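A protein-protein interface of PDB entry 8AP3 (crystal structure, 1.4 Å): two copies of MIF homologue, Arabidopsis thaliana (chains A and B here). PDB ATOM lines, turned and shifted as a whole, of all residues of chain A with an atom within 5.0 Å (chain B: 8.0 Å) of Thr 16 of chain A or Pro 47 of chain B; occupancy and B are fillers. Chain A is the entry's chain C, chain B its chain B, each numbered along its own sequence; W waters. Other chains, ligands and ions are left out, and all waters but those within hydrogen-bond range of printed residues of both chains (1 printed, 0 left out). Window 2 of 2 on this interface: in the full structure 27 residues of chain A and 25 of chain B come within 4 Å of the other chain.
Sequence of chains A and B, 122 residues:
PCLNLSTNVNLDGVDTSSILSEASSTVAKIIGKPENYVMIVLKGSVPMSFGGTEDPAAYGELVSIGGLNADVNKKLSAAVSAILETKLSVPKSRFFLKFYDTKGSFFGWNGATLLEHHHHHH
The side-chain carboxylate (OE2) of Glu 54 of chain B is in hydrogen-bond range of the side-chain hydroxyl (OG) of Ser 17 of chain A, at 2.5 Å.
N of Ser 49 of chain B is in hydrogen-bond range of O of Ile 40 of chain A (2.7 Å).
The backbone NH (N) of Leu 42 of chain A lies within hydrogen-bond range of the backbone carbonyl oxygen (O) of Pro 47 of chain B (3.0 Å).
CB of Pro 47 of chain B touches CG2 of Thr 16 of chain A, at 3.7 Å.
Met 48 of chain B touches Leu 20 of chain A (C to CD1, 3.8 Å).
Ser 49 of chain B touches Leu 20 of chain A (OG to O, 3.9 Å).
Leu 20 of chain A touches Glu 54 of chain B (CD1 to CD, 3.7 Å).
Met 48 of chain B touches Ile 40 of chain A (CA to O, 3.1 Å).
Val 41 of chain A touches Val 46 of chain B.
Pro 47 of chain B touches Val 41 of chain A.
Val 41 of chain A touches Met 48 of chain B.
Leu 42 of chain A touches Val 46 of chain B (O to CG1, 3.99 Å).
Val 46 of chain B touches Lys 43 of chain A (CG1 to CG, 3.6 Å).
SD of Met 48 of chain B lies within hydrogen-bond range of N of Asn 8 of chain B, 3.5 Å away.
The backbone carbonyl oxygen of Glu 54 of chain B is in hydrogen-bond range of the side-chain amide nitrogen of Asn 8 of chain B (3.1 Å).
The side-chain carboxylate (OD1) of Asp 15 of chain A is in hydrogen-bond range of the backbone NH (N) of Ser 17 of chain A, 3.1 Å away.
The backbone carbonyl oxygen (O) of Val 14 of chain A sits at hydrogen-bond distance from the side-chain hydroxyl (OG1) of Thr 16 of chain A, at 3.4 Å.
The backbone carbonyl oxygen (O) of Thr 7 of chain B is in hydrogen-bond range of the backbone NH (N) of Val 46 of chain B (2.9 Å).
No position is printed for both chains.
Of the 13 pairs that touch across the chains among the printed residues, none has its exchanged pair printed and touching as well.
Hydrophobic or aromatic side chains of chain A within 4 Å of the printed part of chain B: Leu 20, Ile 40 and Val 41.
Printed residues of chain B that touch a printed residue of chain A: Val 46, Pro 47, Met 48, Ser 49 and Glu 54.
Hydrophobic or aromatic side chains of chain B that line the printed part of chain A: Val 46, Pro 47 and Met 48.
Among the printed residues, no Asp or Glu carboxylate lies within 4 Å of a Lys or Arg side-chain nitrogen of the other chain.
Of chain B, only Pro 47 (3.7 Å) comes within 4 Å of Thr 16 of chain A.
Of the printed residues of chain B, Leu 20 of chain A touches Met 48 (3.8 Å), Ser 49 (3.9 Å) and Glu 54 (3.7 Å).
Of the printed residues of chain A, Ser 49 of chain B touches Leu 20 and Ile 40.
The nearest residue of chain B that does not touch Thr 16 of chain A is Glu 54 of chain B (5.3 Å).
The nearest residue of chain A that does not touch Pro 47 of chain B is Leu 11 of chain A (4.03 Å).
Water W1 bridges the side-chain carboxylate (OE2) of Glu 54 of chain B and the backbone carbonyl oxygen (O) of Ser 17 of chain A.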
ATOM      1  N   LEU A  11      15.289  12.705 -16.736  1.00  0.00           N
ATOM      2  CA  LEU A  11      15.323  11.867 -17.936  1.00  0.00           C
ATOM      3  C   LEU A  11      15.060  10.400 -17.635  1.00  0.00           C
ATOM      4  O   LEU A  11      14.920   9.626 -18.580  1.00  0.00           O
ATOM      5  CB  LEU A  11      16.670  12.011 -18.632  1.00  0.00           C
ATOM      6  CG  LEU A  11      17.042  13.447 -19.083  1.00  0.00           C
ATOM      7  CD1 LEU A  11      18.405  13.468 -19.755  1.00  0.00           C
ATOM      8  CD2 LEU A  11      15.967  14.067 -19.970  1.00  0.00           C
ATOM      9  N   VAL A  14      11.735   9.695 -19.451  1.00  0.00           N
ATOM     10  CA  VAL A  14      11.513   9.941 -20.869  1.00  0.00           C
ATOM     11  C   VAL A  14      12.452   9.082 -21.700  1.00  0.00           C
ATOM     12  O   VAL A  14      13.529   8.685 -21.256  1.00  0.00           O
ATOM     13  CB  VAL A  14      11.671  11.433 -21.279  1.00  0.00           C
ATOM     14  CG1 VAL A  14      10.833  12.346 -20.408  1.00  0.00           C
ATOM     15  CG2 VAL A  14      13.121  11.854 -21.249  1.00  0.00           C
ATOM     16  N   ASP A  15      12.034   8.814 -22.933  1.00  0.00           N
ATOM     17  CA  ASP A  15      12.894   8.148 -23.908  1.00  0.00           C
ATOM     18  C   ASP A  15      13.916   9.164 -24.400  1.00  0.00           C
ATOM     19  O   ASP A  15      13.653   9.976 -25.287  1.00  0.00           O
ATOM     20  CB  ASP A  15      12.047   7.609 -25.054  1.00  0.00           C
ATOM     21  CG  ASP A  15      12.887   7.102 -26.213  1.00  0.00           C
ATOM     22  OD1 ASP A  15      14.141   7.126 -26.162  1.00  0.00           O
ATOM     23  OD2 ASP A  15      12.263   6.649 -27.195  1.00  0.00           O
ATOM     24  N   THR A  16      15.088   9.119 -23.799  1.00  0.00           N
ATOM     25  CA  THR A  16      16.108  10.112 -24.070  1.00  0.00           C
ATOM     26  C   THR A  16      16.736   9.919 -25.450  1.00  0.00           C
ATOM     27  O   THR A  16      17.117  10.906 -26.105  1.00  0.00           O
ATOM     28  CB  THR A  16      17.145   9.988 -22.964  1.00  0.00           C
ATOM     29  OG1 THR A  16      16.503  10.254 -21.702  1.00  0.00           O
ATOM     30  CG2 THR A  16      18.235  10.986 -23.143  1.00  0.00           C
ATOM     31  N   SER A  17      16.845   8.680 -25.922  1.00  0.00           N
ATOM     32  CA  SER A  17      17.469   8.418 -27.206  1.00  0.00           C
ATOM     33  C   SER A  17      16.642   9.015 -28.327  1.00  0.00           C
ATOM     34  O   SER A  17      17.192   9.474 -29.341  1.00  0.00           O
ATOM     35  CB  SER A  17      17.610   6.909 -27.431  1.00  0.00           C
ATOM     36  OG  SER A  17      18.612   6.376 -26.602  1.00  0.00           O
ATOM     37  N   SER A  18      15.315   9.008 -28.186  1.00  0.00           N
ATOM     38  CA  SER A  18      14.505   9.608 -29.234  1.00  0.00           C
ATOM     39  C   SER A  18      14.697  11.114 -29.289  1.00  0.00           C
ATOM     40  O   SER A  18      14.641  11.686 -30.379  1.00  0.00           O
ATOM     41  CB  SER A  18      13.037   9.231 -29.071  1.00  0.00           C
ATOM     42  OG  SER A  18      12.849   7.884 -29.475  1.00  0.00           O
ATOM     43  N   ILE A  19      14.932  11.774 -28.146  1.00  0.00           N
ATOM     44  CA  ILE A  19      15.237  13.210 -28.153  1.00  0.00           C
ATOM     45  C   ILE A  19      16.554  13.446 -28.854  1.00  0.00           C
ATOM     46  O   ILE A  19      16.660  14.319 -29.724  1.00  0.00           O
ATOM     47  CB  ILE A  19      15.246  13.790 -26.723  1.00  0.00           C
ATOM     48  CG1 ILE A  19      13.880  13.573 -26.065  1.00  0.00           C
ATOM     49  CG2 ILE A  19      15.656  15.304 -26.750  1.00  0.00           C
ATOM     50  CD1 ILE A  19      13.851  13.958 -24.588  1.00  0.00           C
ATOM     51  N   LEU A  20      17.584  12.674 -28.500  1.00  0.00           N
ATOM     52  CA  LEU A  20      18.880  12.821 -29.147  1.00  0.00           C
ATOM     53  C   LEU A  20      18.762  12.644 -30.653  1.00  0.00           C
ATOM     54  O   LEU A  20      19.327  13.426 -31.429  1.00  0.00           O
ATOM     55  CB  LEU A  20      19.886  11.829 -28.578  1.00  0.00           C
ATOM     56  CG  LEU A  20      20.213  11.979 -27.107  1.00  0.00           C
ATOM     57  CD1 LEU A  20      21.115  10.823 -26.705  1.00  0.00           C
ATOM     58  CD2 LEU A  20      20.917  13.298 -26.824  1.00  0.00           C
ATOM     59  N   ILE A  40      24.888  15.785 -30.153  1.00  0.00           N
ATOM     60  CA  ILE A  40      23.859  16.273 -29.242  1.00  0.00           C
ATOM     61  C   ILE A  40      24.219  15.781 -27.852  1.00  0.00           C
ATOM     62  O   ILE A  40      24.535  14.603 -27.686  1.00  0.00           O
ATOM     63  CB  ILE A  40      22.465  15.735 -29.616  1.00  0.00           C
ATOM     64  CG1 ILE A  40      22.167  15.893 -31.122  1.00  0.00           C
ATOM     65  CG2 ILE A  40      21.392  16.425 -28.778  1.00  0.00           C
ATOM     66  CD1 ILE A  40      22.058  17.341 -31.576  1.00  0.00           C
ATOM     67  N   VAL A  41      24.180  16.674 -26.868  1.00  0.00           N
ATOM     68  CA  VAL A  41      24.437  16.366 -25.457  1.00  0.00           C
ATOM     69  C   VAL A  41      23.209  16.799 -24.663  1.00  0.00           C
ATOM     70  O   VAL A  41      22.698  17.908 -24.876  1.00  0.00           O
ATOM     71  CB  VAL A  41      25.691  17.108 -24.952  1.00  0.00           C
ATOM     72  CG1 VAL A  41      25.993  16.710 -23.513  1.00  0.00           C
ATOM     73  CG2 VAL A  41      26.929  16.870 -25.863  1.00  0.00           C
ATOM     74  N   LEU A  42      22.727  15.950 -23.755  1.00  0.00           N
ATOM     75  CA  LEU A  42      21.545  16.300 -22.975  1.00  0.00           C
ATOM     76  C   LEU A  42      21.713  15.847 -21.531  1.00  0.00           C
ATOM     77  O   LEU A  42      21.713  14.649 -21.245  1.00  0.00           O
ATOM     78  CB  LEU A  42      20.299  15.677 -23.594  1.00  0.00           C
ATOM     79  CG  LEU A  42      18.992  15.807 -22.822  1.00  0.00           C
ATOM     80  CD1 LEU A  42      18.605  17.247 -22.575  1.00  0.00           C
ATOM     81  CD2 LEU A  42      17.879  15.101 -23.603  1.00  0.00           C
ATOM     82  N   LYS A  43      21.808  16.804 -20.612  1.00  0.00           N
ATOM     83  CA  LYS A  43      21.909  16.545 -19.180  1.00  0.00           C
ATOM     84  C   LYS A  43      20.569  16.863 -18.545  1.00  0.00           C
ATOM     85  O   LYS A  43      20.015  17.952 -18.757  1.00  0.00           O
ATOM     86  CB  LYS A  43      22.918  17.514 -18.553  1.00  0.00           C
ATOM     87  CG  LYS A  43      24.352  17.207 -18.844  1.00  0.00           C
ATOM     88  CD  LYS A  43      25.206  18.473 -18.777  1.00  0.00           C
ATOM     89  N   SER B   6      32.302  16.676 -21.001  1.00  0.00           N
ATOM     90  CA  SER B   6      31.192  15.768 -20.749  1.00  0.00           C
ATOM     91  C   SER B   6      31.377  14.508 -21.584  1.00  0.00           C
ATOM     92  O   SER B   6      31.868  14.568 -22.716  1.00  0.00           O
ATOM     93  CB  SER B   6      29.839  16.401 -21.147  1.00  0.00           C
ATOM     94  OG  SER B   6      29.534  17.579 -20.393  1.00  0.00           O
ATOM     95  N   THR B   7      30.956  13.372 -21.045  1.00  0.00           N
ATOM     96  CA  THR B   7      31.017  12.115 -21.778  1.00  0.00           C
ATOM     97  C   THR B   7      29.826  11.272 -21.396  1.00  0.00           C
ATOM     98  O   THR B   7      29.307  11.375 -20.286  1.00  0.00           O
ATOM     99  CB  THR B   7      32.344  11.367 -21.497  1.00  0.00           C
ATOM    100  OG1 THR B   7      32.376  10.138 -22.231  1.00  0.00           O
ATOM    101  CG2 THR B   7      32.522  11.036 -20.000  1.00  0.00           C
ATOM    102  N   ASN B   8      29.406  10.414 -22.326  1.00  0.00           N
ATOM    103  CA  ASN B   8      28.420   9.399 -21.995  1.00  0.00           C
ATOM    104  C   ASN B   8      29.004   8.181 -21.272  1.00  0.00           C
ATOM    105  O   ASN B   8      28.228   7.375 -20.741  1.00  0.00           O
ATOM    106  CB  ASN B   8      27.619   8.942 -23.215  1.00  0.00           C
ATOM    107  CG  ASN B   8      28.477   8.528 -24.408  1.00  0.00           C
ATOM    108  OD1 ASN B   8      29.717   8.504 -24.356  1.00  0.00           O
ATOM    109  ND2 ASN B   8      27.796   8.224 -25.524  1.00  0.00           N
ATOM    110  N   VAL B   9      30.329   8.064 -21.190  1.00  0.00           N
ATOM    111  CA  VAL B   9      30.941   6.956 -20.464  1.00  0.00           C
ATOM    112  C   VAL B   9      30.682   7.106 -18.967  1.00  0.00           C
ATOM    113  O   VAL B   9      30.759   8.210 -18.410  1.00  0.00           O
ATOM    114  CB  VAL B   9      32.443   6.912 -20.793  1.00  0.00           C
ATOM    115  CG1 VAL B   9      33.155   5.852 -19.973  1.00  0.00           C
ATOM    116  CG2 VAL B   9      32.638   6.634 -22.287  1.00  0.00           C
ATOM    117  N   GLY B  44      30.463  12.584 -16.283  1.00  0.00           N
ATOM    118  CA  GLY B  44      30.206  11.323 -16.937  1.00  0.00           C
ATOM    119  C   GLY B  44      28.730  10.960 -16.943  1.00  0.00           C
ATOM    120  O   GLY B  44      27.867  11.646 -16.388  1.00  0.00           O
ATOM    121  N   SER B  45      28.451   9.845 -17.609  1.00  0.00           N
ATOM    122  CA  SER B  45      27.084   9.319 -17.725  1.00  0.00           C
ATOM    123  C   SER B  45      26.100  10.330 -18.316  1.00  0.00           C
ATOM    124  O   SER B  45      24.899  10.280 -18.012  1.00  0.00           O
ATOM    125  CB  SER B  45      26.538   8.782 -16.397  1.00  0.00           C
ATOM    126  OG  SER B  45      27.395   7.762 -15.916  1.00  0.00           O
ATOM    127  N   VAL B  46      26.574  11.200 -19.209  1.00  0.00           N
ATOM    128  CA  VAL B  46      25.741  12.233 -19.822  1.00  0.00           C
ATOM    129  C   VAL B  46      25.210  11.706 -21.156  1.00  0.00           C
ATOM    130  O   VAL B  46      26.014  11.355 -22.029  1.00  0.00           O
ATOM    131  CB  VAL B  46      26.551  13.507 -20.070  1.00  0.00           C
ATOM    132  CG1 VAL B  46      25.675  14.512 -20.797  1.00  0.00           C
ATOM    133  CG2 VAL B  46      27.048  14.082 -18.752  1.00  0.00           C
ATOM    134  N   PRO B  47      23.874  11.599 -21.344  1.00  0.00           N
ATOM    135  CA  PRO B  47      23.316  11.161 -22.619  1.00  0.00           C
ATOM    136  C   PRO B  47      23.898  11.993 -23.764  1.00  0.00           C
ATOM    137  O   PRO B  47      23.845  13.205 -23.699  1.00  0.00           O
ATOM    138  CB  PRO B  47      21.820  11.458 -22.481  1.00  0.00           C
ATOM    139  CG  PRO B  47      21.561  11.299 -21.007  1.00  0.00           C
ATOM    140  CD  PRO B  47      22.809  11.854 -20.356  1.00  0.00           C
ATOM    141  N   MET B  48      24.428  11.319 -24.781  1.00  0.00           N
ATOM    142  CA  MET B  48      24.910  12.105 -25.939  1.00  0.00           C
ATOM    143  C   MET B  48      24.897  11.279 -27.221  1.00  0.00           C
ATOM    144  O   MET B  48      24.967  10.040 -27.139  1.00  0.00           O
ATOM    145  CB  MET B  48      26.316  12.677 -25.711  1.00  0.00           C
ATOM    146  CG  MET B  48      27.364  11.695 -25.269  1.00  0.00           C
ATOM    147  SD  MET B  48      28.899  12.611 -24.963  1.00  0.00           S
ATOM    148  CE  MET B  48      28.371  13.713 -23.654  1.00  0.00           C
ATOM    149  N   SER B  49      24.743  11.960 -28.348  1.00  0.00           N
ATOM    150  CA  SER B  49      24.801  11.274 -29.666  1.00  0.00           C
ATOM    151  C   SER B  49      25.824  11.980 -30.586  1.00  0.00           C
ATOM    152  O   SER B  49      26.097  13.269 -30.645  1.00  0.00           O
ATOM    153  CB  SER B  49      23.444  11.230 -30.309  1.00  0.00           C
ATOM    154  OG  SER B  49      23.049  12.522 -30.741  1.00  0.00           O
ATOM    155  N   GLU B  54      25.065   6.372 -30.138  1.00  0.00           N
ATOM    156  CA  GLU B  54      25.355   6.625 -28.737  1.00  0.00           C
ATOM    157  C   GLU B  54      26.563   5.849 -28.225  1.00  0.00           C
ATOM    158  O   GLU B  54      26.734   5.696 -27.013  1.00  0.00           O
ATOM    159  CB  GLU B  54      24.120   6.370 -27.880  1.00  0.00           C
ATOM    160  CG  GLU B  54      23.004   7.320 -28.196  1.00  0.00           C
ATOM    161  CD  GLU B  54      21.870   7.205 -27.216  1.00  0.00           C
ATOM    162  OE1 GLU B  54      22.121   7.181 -25.985  1.00  0.00           O
ATOM    163  OE2 GLU B  54      20.739   7.192 -27.700  1.00  0.00           O
HETATM  164  O   HOH W   1      20.036   8.552 -30.194  1.00  0.00           O
